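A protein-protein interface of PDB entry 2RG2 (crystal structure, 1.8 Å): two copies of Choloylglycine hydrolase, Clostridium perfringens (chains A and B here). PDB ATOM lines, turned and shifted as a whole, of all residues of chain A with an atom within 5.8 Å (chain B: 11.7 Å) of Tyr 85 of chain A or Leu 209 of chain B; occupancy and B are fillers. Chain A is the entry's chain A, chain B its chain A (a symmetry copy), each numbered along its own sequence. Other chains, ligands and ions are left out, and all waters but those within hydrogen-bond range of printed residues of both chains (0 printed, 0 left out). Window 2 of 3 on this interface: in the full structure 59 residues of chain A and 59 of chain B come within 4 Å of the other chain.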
ATOM      1  N   PHE A  82     -25.769   5.224   7.647  1.00  0.00           N
ATOM      2  CA  PHE A  82     -25.443   5.771   6.321  1.00  0.00           C
ATOM      3  C   PHE A  82     -24.504   6.991   6.475  1.00  0.00           C
ATOM      4  O   PHE A  82     -24.888   8.128   6.170  1.00  0.00           O
ATOM      5  CB  PHE A  82     -26.752   6.136   5.603  1.00  0.00           C
ATOM      6  CG  PHE A  82     -26.604   6.517   4.147  1.00  0.00           C
ATOM      7  CD1 PHE A  82     -25.888   5.725   3.251  1.00  0.00           C
ATOM      8  CD2 PHE A  82     -27.272   7.641   3.656  1.00  0.00           C
ATOM      9  CE1 PHE A  82     -25.788   6.075   1.886  1.00  0.00           C
ATOM     10  CE2 PHE A  82     -27.183   8.000   2.295  1.00  0.00           C
ATOM     11  CZ  PHE A  82     -26.430   7.217   1.410  1.00  0.00           C
ATOM     12  N   PRO A  83     -23.261   6.758   6.947  1.00  0.00           N
ATOM     13  CA  PRO A  83     -22.351   7.883   7.167  1.00  0.00           C
ATOM     14  C   PRO A  83     -21.762   8.471   5.877  1.00  0.00           C
ATOM     15  O   PRO A  83     -21.795   7.831   4.831  1.00  0.00           O
ATOM     16  CB  PRO A  83     -21.250   7.277   8.048  1.00  0.00           C
ATOM     17  CG  PRO A  83     -21.242   5.798   7.709  1.00  0.00           C
ATOM     18  CD  PRO A  83     -22.658   5.453   7.296  1.00  0.00           C
ATOM     19  N   VAL A  84     -21.246   9.699   5.968  1.00  0.00           N
ATOM     20  CA  VAL A  84     -20.520  10.374   4.873  1.00  0.00           C
ATOM     21  C   VAL A  84     -21.382  10.873   3.708  1.00  0.00           C
ATOM     22  O   VAL A  84     -21.315  12.057   3.360  1.00  0.00           O
ATOM     23  CB  VAL A  84     -19.347   9.511   4.304  1.00  0.00           C
ATOM     24  CG1 VAL A  84     -18.651  10.233   3.161  1.00  0.00           C
ATOM     25  CG2 VAL A  84     -18.351   9.161   5.409  1.00  0.00           C
ATOM     26  N   TYR A  85     -22.157   9.975   3.094  1.00  0.00           N
ATOM     27  CA  TYR A  85     -22.892  10.290   1.866  1.00  0.00           C
ATOM     28  C   TYR A  85     -24.282  10.875   2.116  1.00  0.00           C
ATOM     29  O   TYR A  85     -24.906  11.404   1.190  1.00  0.00           O
ATOM     30  CB  TYR A  85     -22.959   9.074   0.919  1.00  0.00           C
ATOM     31  CG  TYR A  85     -21.584   8.617   0.480  1.00  0.00           C
ATOM     32  CD1 TYR A  85     -20.905   9.267  -0.551  1.00  0.00           C
ATOM     33  CD2 TYR A  85     -20.939   7.571   1.135  1.00  0.00           C
ATOM     34  CE1 TYR A  85     -19.621   8.871  -0.938  1.00  0.00           C
ATOM     35  CE2 TYR A  85     -19.657   7.163   0.756  1.00  0.00           C
ATOM     36  CZ  TYR A  85     -19.005   7.812  -0.278  1.00  0.00           C
ATOM     37  OH  TYR A  85     -17.735   7.402  -0.646  1.00  0.00           O
ATOM     38  N   VAL A  86     -24.764  10.774   3.351  1.00  0.00           N
ATOM     39  CA  VAL A  86     -26.071  11.330   3.702  1.00  0.00           C
ATOM     40  C   VAL A  86     -25.988  12.848   3.809  1.00  0.00           C
ATOM     41  O   VAL A  86     -24.934  13.399   4.150  1.00  0.00           O
ATOM     42  CB  VAL A  86     -26.644  10.729   5.025  1.00  0.00           C
ATOM     43  CG1 VAL A  86     -25.971  11.326   6.258  1.00  0.00           C
ATOM     44  CG2 VAL A  86     -28.158  10.912   5.087  1.00  0.00           C
ATOM     45  N   SER A  87     -27.095  13.517   3.496  1.00  0.00           N
ATOM     46  CA  SER A  87     -27.213  14.948   3.743  1.00  0.00           C
ATOM     47  C   SER A  87     -28.637  15.295   4.119  1.00  0.00           C
ATOM     48  O   SER A  87     -29.551  15.104   3.319  1.00  0.00           O
ATOM     49  CB  SER A  87     -26.806  15.759   2.520  1.00  0.00           C
ATOM     50  OG  SER A  87     -26.983  17.150   2.779  1.00  0.00           O
ATOM     51  N   GLN A 157     -31.182  10.115   1.300  1.00  0.00           N
ATOM     52  CA  GLN A 157     -31.061  11.545   1.037  1.00  0.00           C
ATOM     53  C   GLN A 157     -29.618  11.971   0.915  1.00  0.00           C
ATOM     54  O   GLN A 157     -28.853  11.877   1.872  1.00  0.00           O
ATOM     55  CB  GLN A 157     -31.747  12.401   2.084  1.00  0.00           C
ATOM     56  CG  GLN A 157     -31.841  13.854   1.590  1.00  0.00           C
ATOM     57  CD  GLN A 157     -32.901  14.630   2.286  1.00  0.00           C
ATOM     58  OE1 GLN A 157     -34.080  14.261   2.242  1.00  0.00           O
ATOM     59  NE2 GLN A 157     -32.500  15.728   2.944  1.00  0.00           N
ATOM     60  N   THR A 158     -29.266  12.456  -0.272  1.00  0.00           N
ATOM     61  CA  THR A 158     -27.965  13.073  -0.506  1.00  0.00           C
ATOM     62  C   THR A 158     -28.122  14.598  -0.595  1.00  0.00           C
ATOM     63  O   THR A 158     -29.230  15.121  -0.488  1.00  0.00           O
ATOM     64  CB  THR A 158     -27.350  12.560  -1.800  1.00  0.00           C
ATOM     65  OG1 THR A 158     -28.197  12.920  -2.902  1.00  0.00           O
ATOM     66  CG2 THR A 158     -27.176  11.034  -1.746  1.00  0.00           C
ATOM     67  N   LYS A 159     -27.019  15.313  -0.807  1.00  0.00           N
ATOM     68  CA  LYS A 159     -27.097  16.767  -0.993  1.00  0.00           C
ATOM     69  C   LYS A 159     -27.809  17.128  -2.304  1.00  0.00           C
ATOM     70  O   LYS A 159     -28.358  18.221  -2.438  1.00  0.00           O
ATOM     71  CB  LYS A 159     -25.705  17.412  -0.923  1.00  0.00           C
ATOM     72  CG  LYS A 159     -24.706  16.861  -1.930  1.00  0.00           C
ATOM     73  CD  LYS A 159     -23.537  17.805  -2.155  1.00  0.00           C
ATOM     74  CE  LYS A 159     -22.412  17.088  -2.886  1.00  0.00           C
ATOM     75  NZ  LYS A 159     -21.120  17.817  -2.754  1.00  0.00           N
ATOM     76  N   ASN A 174     -24.658  -0.445   4.442  1.00  0.00           N
ATOM     77  CA  ASN A 174     -24.354   0.933   4.822  1.00  0.00           C
ATOM     78  C   ASN A 174     -23.690   1.627   3.641  1.00  0.00           C
ATOM     79  O   ASN A 174     -23.917   1.216   2.507  1.00  0.00           O
ATOM     80  CB  ASN A 174     -23.523   0.957   6.105  1.00  0.00           C
ATOM     81  CG  ASN A 174     -24.093   0.027   7.174  1.00  0.00           C
ATOM     82  OD1 ASN A 174     -23.551  -1.056   7.422  1.00  0.00           O
ATOM     83  ND2 ASN A 174     -25.228   0.418   7.767  1.00  0.00           N
ATOM     84  N   SER A 175     -22.902   2.667   3.891  1.00  0.00           N
ATOM     85  CA  SER A 175     -22.241   3.415   2.814  1.00  0.00           C
ATOM     86  C   SER A 175     -21.274   2.538   2.012  1.00  0.00           C
ATOM     87  O   SER A 175     -20.766   1.543   2.547  1.00  0.00           O
ATOM     88  CB  SER A 175     -21.534   4.627   3.414  1.00  0.00           C
ATOM     89  OG  SER A 175     -22.515   5.440   4.037  1.00  0.00           O
ATOM     90  N   PRO A 176     -21.018   2.885   0.729  1.00  0.00           N
ATOM     91  CA  PRO A 176     -21.540   4.025  -0.037  1.00  0.00           C
ATOM     92  C   PRO A 176     -23.017   3.922  -0.443  1.00  0.00           C
ATOM     93  O   PRO A 176     -23.770   3.100   0.077  1.00  0.00           O
ATOM     94  CB  PRO A 176     -20.640   4.059  -1.288  1.00  0.00           C
ATOM     95  CG  PRO A 176     -19.522   3.106  -1.031  1.00  0.00           C
ATOM     96  CD  PRO A 176     -20.073   2.092  -0.073  1.00  0.00           C
ATOM     97  N   THR A 177     -23.430   4.801  -1.354  1.00  0.00           N
ATOM     98  CA  THR A 177     -24.805   4.854  -1.839  1.00  0.00           C
ATOM     99  C   THR A 177     -25.250   3.548  -2.502  1.00  0.00           C
ATOM    100  O   THR A 177     -24.413   2.728  -2.937  1.00  0.00           O
ATOM    101  CB  THR A 177     -24.988   6.018  -2.838  1.00  0.00           C
ATOM    102  OG1 THR A 177     -24.133   5.807  -3.975  1.00  0.00           O
ATOM    103  CG2 THR A 177     -24.647   7.361  -2.175  1.00  0.00           C
ATOM    104  N   TRP A 180     -23.950   2.517  -5.826  1.00  0.00           N
ATOM    105  CA  TRP A 180     -22.550   2.096  -5.738  1.00  0.00           C
ATOM    106  C   TRP A 180     -22.495   0.576  -5.496  1.00  0.00           C
ATOM    107  O   TRP A 180     -21.748  -0.146  -6.159  1.00  0.00           O
ATOM    108  CB  TRP A 180     -21.772   2.862  -4.650  1.00  0.00           C
ATOM    109  CG  TRP A 180     -20.302   2.504  -4.644  1.00  0.00           C
ATOM    110  CD1 TRP A 180     -19.292   3.192  -5.246  1.00  0.00           C
ATOM    111  CD2 TRP A 180     -19.695   1.331  -4.062  1.00  0.00           C
ATOM    112  NE1 TRP A 180     -18.091   2.532  -5.076  1.00  0.00           N
ATOM    113  CE2 TRP A 180     -18.310   1.392  -4.349  1.00  0.00           C
ATOM    114  CE3 TRP A 180     -20.184   0.259  -3.302  1.00  0.00           C
ATOM    115  CZ2 TRP A 180     -17.399   0.418  -3.896  1.00  0.00           C
ATOM    116  CZ3 TRP A 180     -19.276  -0.741  -2.886  1.00  0.00           C
ATOM    117  CH2 TRP A 180     -17.905  -0.638  -3.182  1.00  0.00           C
ATOM    118  N   PRO A 224     -19.258  -2.702   5.162  1.00  0.00           N
ATOM    119  CA  PRO A 224     -20.547  -2.655   4.469  1.00  0.00           C
ATOM    120  C   PRO A 224     -20.518  -3.241   3.072  1.00  0.00           C
ATOM    121  O   PRO A 224     -21.441  -3.953   2.698  1.00  0.00           O
ATOM    122  CB  PRO A 224     -20.888  -1.146   4.442  1.00  0.00           C
ATOM    123  CG  PRO A 224     -20.162  -0.578   5.642  1.00  0.00           C
ATOM    124  CD  PRO A 224     -18.862  -1.375   5.679  1.00  0.00           C
ATOM    125  N   ALA A 225     -19.492  -2.934   2.274  1.00  0.00           N
ATOM    126  CA  ALA A 225     -19.464  -3.458   0.912  1.00  0.00           C
ATOM    127  C   ALA A 225     -19.354  -4.980   0.870  1.00  0.00           C
ATOM    128  O   ALA A 225     -20.042  -5.627   0.106  1.00  0.00           O
ATOM    129  CB  ALA A 225     -18.326  -2.817   0.097  1.00  0.00           C
ATOM    130  N   GLN B 195     -10.315  -0.813  14.135  1.00  0.00           N
ATOM    131  CA  GLN B 195     -10.712   0.036  13.009  1.00  0.00           C
ATOM    132  C   GLN B 195      -9.559   0.874  12.474  1.00  0.00           C
ATOM    133  O   GLN B 195      -8.774   1.444  13.250  1.00  0.00           O
ATOM    134  CB  GLN B 195     -11.875   0.951  13.426  1.00  0.00           C
ATOM    135  CG  GLN B 195     -12.425   1.893  12.328  1.00  0.00           C
ATOM    136  CD  GLN B 195     -13.154   1.168  11.199  1.00  0.00           C
ATOM    137  OE1 GLN B 195     -12.995  -0.045  11.004  1.00  0.00           O
ATOM    138  NE2 GLN B 195     -13.941   1.920  10.434  1.00  0.00           N
ATOM    139  N   VAL B 196      -9.468   0.935  11.140  1.00  0.00           N
ATOM    140  CA  VAL B 196      -8.611   1.909  10.452  1.00  0.00           C
ATOM    141  C   VAL B 196      -9.527   2.974   9.843  1.00  0.00           C
ATOM    142  O   VAL B 196     -10.143   2.733   8.813  1.00  0.00           O
ATOM    143  CB  VAL B 196      -7.752   1.250   9.343  1.00  0.00           C
ATOM    144  CG1 VAL B 196      -6.757   2.265   8.771  1.00  0.00           C
ATOM    145  CG2 VAL B 196      -7.003   0.045   9.888  1.00  0.00           C
ATOM    146  N   PRO B 197      -9.636   4.154  10.494  1.00  0.00           N
ATOM    147  CA  PRO B 197     -10.676   5.118  10.119  1.00  0.00           C
ATOM    148  C   PRO B 197     -10.363   5.924   8.858  1.00  0.00           C
ATOM    149  O   PRO B 197     -11.291   6.429   8.206  1.00  0.00           O
ATOM    150  CB  PRO B 197     -10.726   6.063  11.326  1.00  0.00           C
ATOM    151  CG  PRO B 197      -9.369   6.007  11.912  1.00  0.00           C
ATOM    152  CD  PRO B 197      -8.810   4.639  11.618  1.00  0.00           C
ATOM    153  N   GLU B 198      -9.078   6.064   8.536  1.00  0.00           N
ATOM    154  CA  GLU B 198      -8.676   6.858   7.364  1.00  0.00           C
ATOM    155  C   GLU B 198      -7.293   6.516   6.804  1.00  0.00           C
ATOM    156  O   GLU B 198      -6.486   5.837   7.452  1.00  0.00           O
ATOM    157  CB  GLU B 198      -8.764   8.357   7.676  1.00  0.00           C
ATOM    158  CG  GLU B 198      -7.716   8.860   8.655  1.00  0.00           C
ATOM    159  CD  GLU B 198      -7.697  10.376   8.752  1.00  0.00           C
ATOM    160  OE1 GLU B 198      -7.822  11.059   7.702  1.00  0.00           O
ATOM    161  OE2 GLU B 198      -7.546  10.888   9.883  1.00  0.00           O
ATOM    162  N   PHE B 199      -7.027   7.018   5.599  1.00  0.00           N
ATOM    163  CA  PHE B 199      -5.762   6.798   4.906  1.00  0.00           C
ATOM    164  C   PHE B 199      -5.547   8.017   4.019  1.00  0.00           C
ATOM    165  O   PHE B 199      -6.437   8.403   3.249  1.00  0.00           O
ATOM    166  CB  PHE B 199      -5.853   5.522   4.060  1.00  0.00           C
ATOM    167  CG  PHE B 199      -4.558   5.108   3.401  1.00  0.00           C
ATOM    168  CD1 PHE B 199      -4.091   5.754   2.254  1.00  0.00           C
ATOM    169  CD2 PHE B 199      -3.835   4.031   3.897  1.00  0.00           C
ATOM    170  CE1 PHE B 199      -2.902   5.351   1.642  1.00  0.00           C
ATOM    171  CE2 PHE B 199      -2.648   3.617   3.287  1.00  0.00           C
ATOM    172  CZ  PHE B 199      -2.183   4.281   2.149  1.00  0.00           C
ATOM    173  N   GLN B 204      -5.692  12.884  -2.028  1.00  0.00           N
ATOM    174  CA  GLN B 204      -7.024  12.326  -1.834  1.00  0.00           C
ATOM    175  C   GLN B 204      -7.132  11.805  -0.409  1.00  0.00           C
ATOM    176  O   GLN B 204      -6.306  11.002   0.024  1.00  0.00           O
ATOM    177  CB  GLN B 204      -7.283  11.191  -2.836  1.00  0.00           C
ATOM    178  CG  GLN B 204      -8.658  10.501  -2.708  1.00  0.00           C
ATOM    179  CD  GLN B 204      -9.812  11.359  -3.205  1.00  0.00           C
ATOM    180  OE1 GLN B 204      -9.677  12.123  -4.164  1.00  0.00           O
ATOM    181  NE2 GLN B 204     -10.959  11.230  -2.553  1.00  0.00           N
ATOM    182  N   SER B 205      -8.140  12.281   0.320  1.00  0.00           N
ATOM    183  CA  SER B 205      -8.428  11.780   1.663  1.00  0.00           C
ATOM    184  C   SER B 205      -9.348  10.579   1.543  1.00  0.00           C
ATOM    185  O   SER B 205     -10.412  10.677   0.936  1.00  0.00           O
ATOM    186  CB  SER B 205      -9.110  12.864   2.515  1.00  0.00           C
ATOM    187  OG  SER B 205      -8.179  13.854   2.945  1.00  0.00           O
ATOM    188  N   LEU B 206      -8.934   9.446   2.111  1.00  0.00           N
ATOM    189  CA  LEU B 206      -9.774   8.244   2.127  1.00  0.00           C
ATOM    190  C   LEU B 206     -10.359   8.050   3.511  1.00  0.00           C
ATOM    191  O   LEU B 206      -9.656   8.198   4.510  1.00  0.00           O
ATOM    192  CB  LEU B 206      -8.971   6.997   1.748  1.00  0.00           C
ATOM    193  CG  LEU B 206      -8.192   7.047   0.437  1.00  0.00           C
ATOM    194  CD1 LEU B 206      -7.450   5.729   0.222  1.00  0.00           C
ATOM    195  CD2 LEU B 206      -9.149   7.335  -0.714  1.00  0.00           C
ATOM    196  N   THR B 207     -11.636   7.694   3.560  1.00  0.00           N
ATOM    197  CA  THR B 207     -12.342   7.535   4.835  1.00  0.00           C
ATOM    198  C   THR B 207     -13.034   6.176   4.915  1.00  0.00           C
ATOM    199  O   THR B 207     -13.703   5.752   3.966  1.00  0.00           O
ATOM    200  CB  THR B 207     -13.368   8.696   5.079  1.00  0.00           C
ATOM    201  OG1 THR B 207     -14.138   8.431   6.261  1.00  0.00           O
ATOM    202  CG2 THR B 207     -14.335   8.828   3.931  1.00  0.00           C
ATOM    203  N   ALA B 208     -12.873   5.493   6.045  1.00  0.00           N
ATOM    204  CA  ALA B 208     -13.573   4.229   6.272  1.00  0.00           C
ATOM    205  C   ALA B 208     -15.075   4.432   6.116  1.00  0.00           C
ATOM    206  O   ALA B 208     -15.649   5.330   6.731  1.00  0.00           O
ATOM    207  CB  ALA B 208     -13.264   3.691   7.658  1.00  0.00           C
ATOM    208  N   LEU B 209     -15.696   3.582   5.302  1.00  0.00           N
ATOM    209  CA  LEU B 209     -17.134   3.652   5.018  1.00  0.00           C
ATOM    210  C   LEU B 209     -17.988   3.009   6.114  1.00  0.00           C
ATOM    211  O   LEU B 209     -19.205   3.196   6.163  1.00  0.00           O
ATOM    212  CB  LEU B 209     -17.424   2.973   3.680  1.00  0.00           C
ATOM    213  CG  LEU B 209     -16.713   3.567   2.452  1.00  0.00           C
ATOM    214  CD1 LEU B 209     -16.557   2.529   1.390  1.00  0.00           C
ATOM    215  CD2 LEU B 209     -17.481   4.728   1.907  1.00  0.00           C
ATOM    216  N   GLY B 210     -17.345   2.221   6.967  1.00  0.00           N
ATOM    217  CA  GLY B 210     -18.000   1.565   8.083  1.00  0.00           C
ATOM    218  C   GLY B 210     -16.949   0.831   8.889  1.00  0.00           C
ATOM    219  O   GLY B 210     -15.761   0.864   8.548  1.00  0.00           O
ATOM    220  N   GLN B 211     -17.381   0.162   9.954  1.00  0.00           N
ATOM    221  CA  GLN B 211     -16.459  -0.585  10.789  1.00  0.00           C
ATOM    222  C   GLN B 211     -15.957  -1.809  10.036  1.00  0.00           C
ATOM    223  O   GLN B 211     -16.661  -2.342   9.166  1.00  0.00           O
ATOM    224  CB  GLN B 211     -17.150  -1.020  12.085  1.00  0.00           C
ATOM    225  CG  GLN B 211     -17.475   0.131  13.025  1.00  0.00           C
ATOM    226  CD  GLN B 211     -16.225   0.783  13.616  1.00  0.00           C
ATOM    227  OE1 GLN B 211     -16.215   1.981  13.882  1.00  0.00           O
ATOM    228  NE2 GLN B 211     -15.177  -0.009  13.832  1.00  0.00           N
ATOM    229  N   GLY B 212     -14.747  -2.249  10.368  1.00  0.00           N
ATOM    230  CA  GLY B 212     -14.219  -3.506   9.823  1.00  0.00           C
ATOM    231  C   GLY B 212     -13.084  -3.382   8.822  1.00  0.00           C
ATOM    232  O   GLY B 212     -12.622  -4.386   8.274  1.00  0.00           O
ATOM    233  N   THR B 213     -12.602  -2.163   8.594  1.00  0.00           N
ATOM    234  CA  THR B 213     -11.563  -1.974   7.572  1.00  0.00           C
ATOM    235  C   THR B 213     -10.237  -2.690   7.857  1.00  0.00           C
ATOM    236  O   THR B 213      -9.449  -2.933   6.938  1.00  0.00           O
ATOM    237  CB  THR B 213     -11.298  -0.489   7.296  1.00  0.00           C
ATOM    238  OG1 THR B 213     -10.939   0.164   8.518  1.00  0.00           O
ATOM    239  CG2 THR B 213     -12.570   0.159   6.727  1.00  0.00           C
ATOM    240  N   GLY B 214      -9.985  -3.005   9.124  1.00  0.00           N
ATOM    241  CA  GLY B 214      -8.744  -3.684   9.515  1.00  0.00           C
ATOM    242  C   GLY B 214      -8.620  -5.126   9.023  1.00  0.00           C
ATOM    243  O   GLY B 214      -7.506  -5.647   8.898  1.00  0.00           O
ATOM    244  N   LEU B 215      -9.763  -5.770   8.740  1.00  0.00           N
ATOM    245  CA  LEU B 215      -9.799  -7.180   8.307  1.00  0.00           C
ATOM    246  C   LEU B 215      -9.997  -7.399   6.810  1.00  0.00           C
ATOM    247  O   LEU B 215     -10.212  -8.520   6.354  1.00  0.00           O
ATOM    248  CB  LEU B 215     -10.884  -7.954   9.079  1.00  0.00           C
ATOM    249  CG  LEU B 215     -10.723  -8.220  10.573  1.00  0.00           C
ATOM    250  CD1 LEU B 215     -11.882  -9.116  11.067  1.00  0.00           C
ATOM    251  CD2 LEU B 215      -9.373  -8.869  10.887  1.00  0.00           C
ATOM    252  N   VAL B 216      -9.932  -6.326   6.027  1.00  0.00           N
ATOM    253  CA  VAL B 216     -10.040  -6.462   4.580  1.00  0.00           C
ATOM    254  C   VAL B 216      -8.878  -7.363   4.138  1.00  0.00           C
ATOM    255  O   VAL B 216      -7.733  -7.146   4.531  1.00  0.00           O
ATOM    256  CB  VAL B 216     -10.082  -5.069   3.888  1.00  0.00           C
ATOM    257  CG1 VAL B 216      -9.972  -5.191   2.380  1.00  0.00           C
ATOM    258  CG2 VAL B 216     -11.379  -4.327   4.286  1.00  0.00           C
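The backbone carbonyl oxygen of Pro 83 of chain A lies within hydrogen-bond range of the side-chain hydroxyl of Ser 175 of chain A, at 2.6 Å.
O of Gly 210 of chain B is in hydrogen-bond range of NE2 of Gln 195 of chain B (2.8 Å).
CG of Pro 83 of chain A touches O of Leu 209 of chain B, at 3.6 Å.
CE2 of Tyr 85 of chain A touches CD2 of Leu 209 of chain B, at 3.5 Å.
Ser 175 of chain A touches Leu 209 of chain B.
Pro 176 of chain A touches Leu 209 of chain B.
Pro 224 of chain A touches Leu 209 of chain B (CG to O, 3.9 Å).
CD of Pro 224 of chain A touches CA of Gly 210 of chain B, at 3.9 Å.
Of the printed residues of chain B, Tyr 85 of chain A touches Leu 209.
No residue of chain B comes within 4 Å of Phe 82 of chain A.
Pro 83 of chain A touches just one residue of chain B: Leu 209.
Val 84 of chain A touches none of the printed residues of chain B.
No residue of chain B comes within 4 Å of Val 86 of chain A.
No residue of chain B comes within 4 Å of Thr 158 of chain A.
No residue of chain B comes within 4 Å of Asn 174 of chain A.
Ser 175 of chain A touches one residue of chain B.
No residue of chain B comes within 4 Å of Thr 177 of chain A.
Printed residues of chain B within 4 Å of Pro 224 of chain A: Leu 209 and Gly 210.
Printed residues of chain A within 4 Å of Gly 210 of chain B: Pro 224.
Lys 159 of chain A touches none of the printed residues of chain B.
Ala 208 of chain B touches none of the printed residues of chain A.
Of the 18 printed residues of chain B, 2 touch a printed residue of chain A.
Hydrophobic or aromatic side chains of chain B within 4 Å of the printed part of chain A: Leu 209.
Among the printed residues, no Asp or Glu carboxylate lies within 4 Å of a Lys or Arg side-chain nitrogen of the other chain.
No position is printed for both chains.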
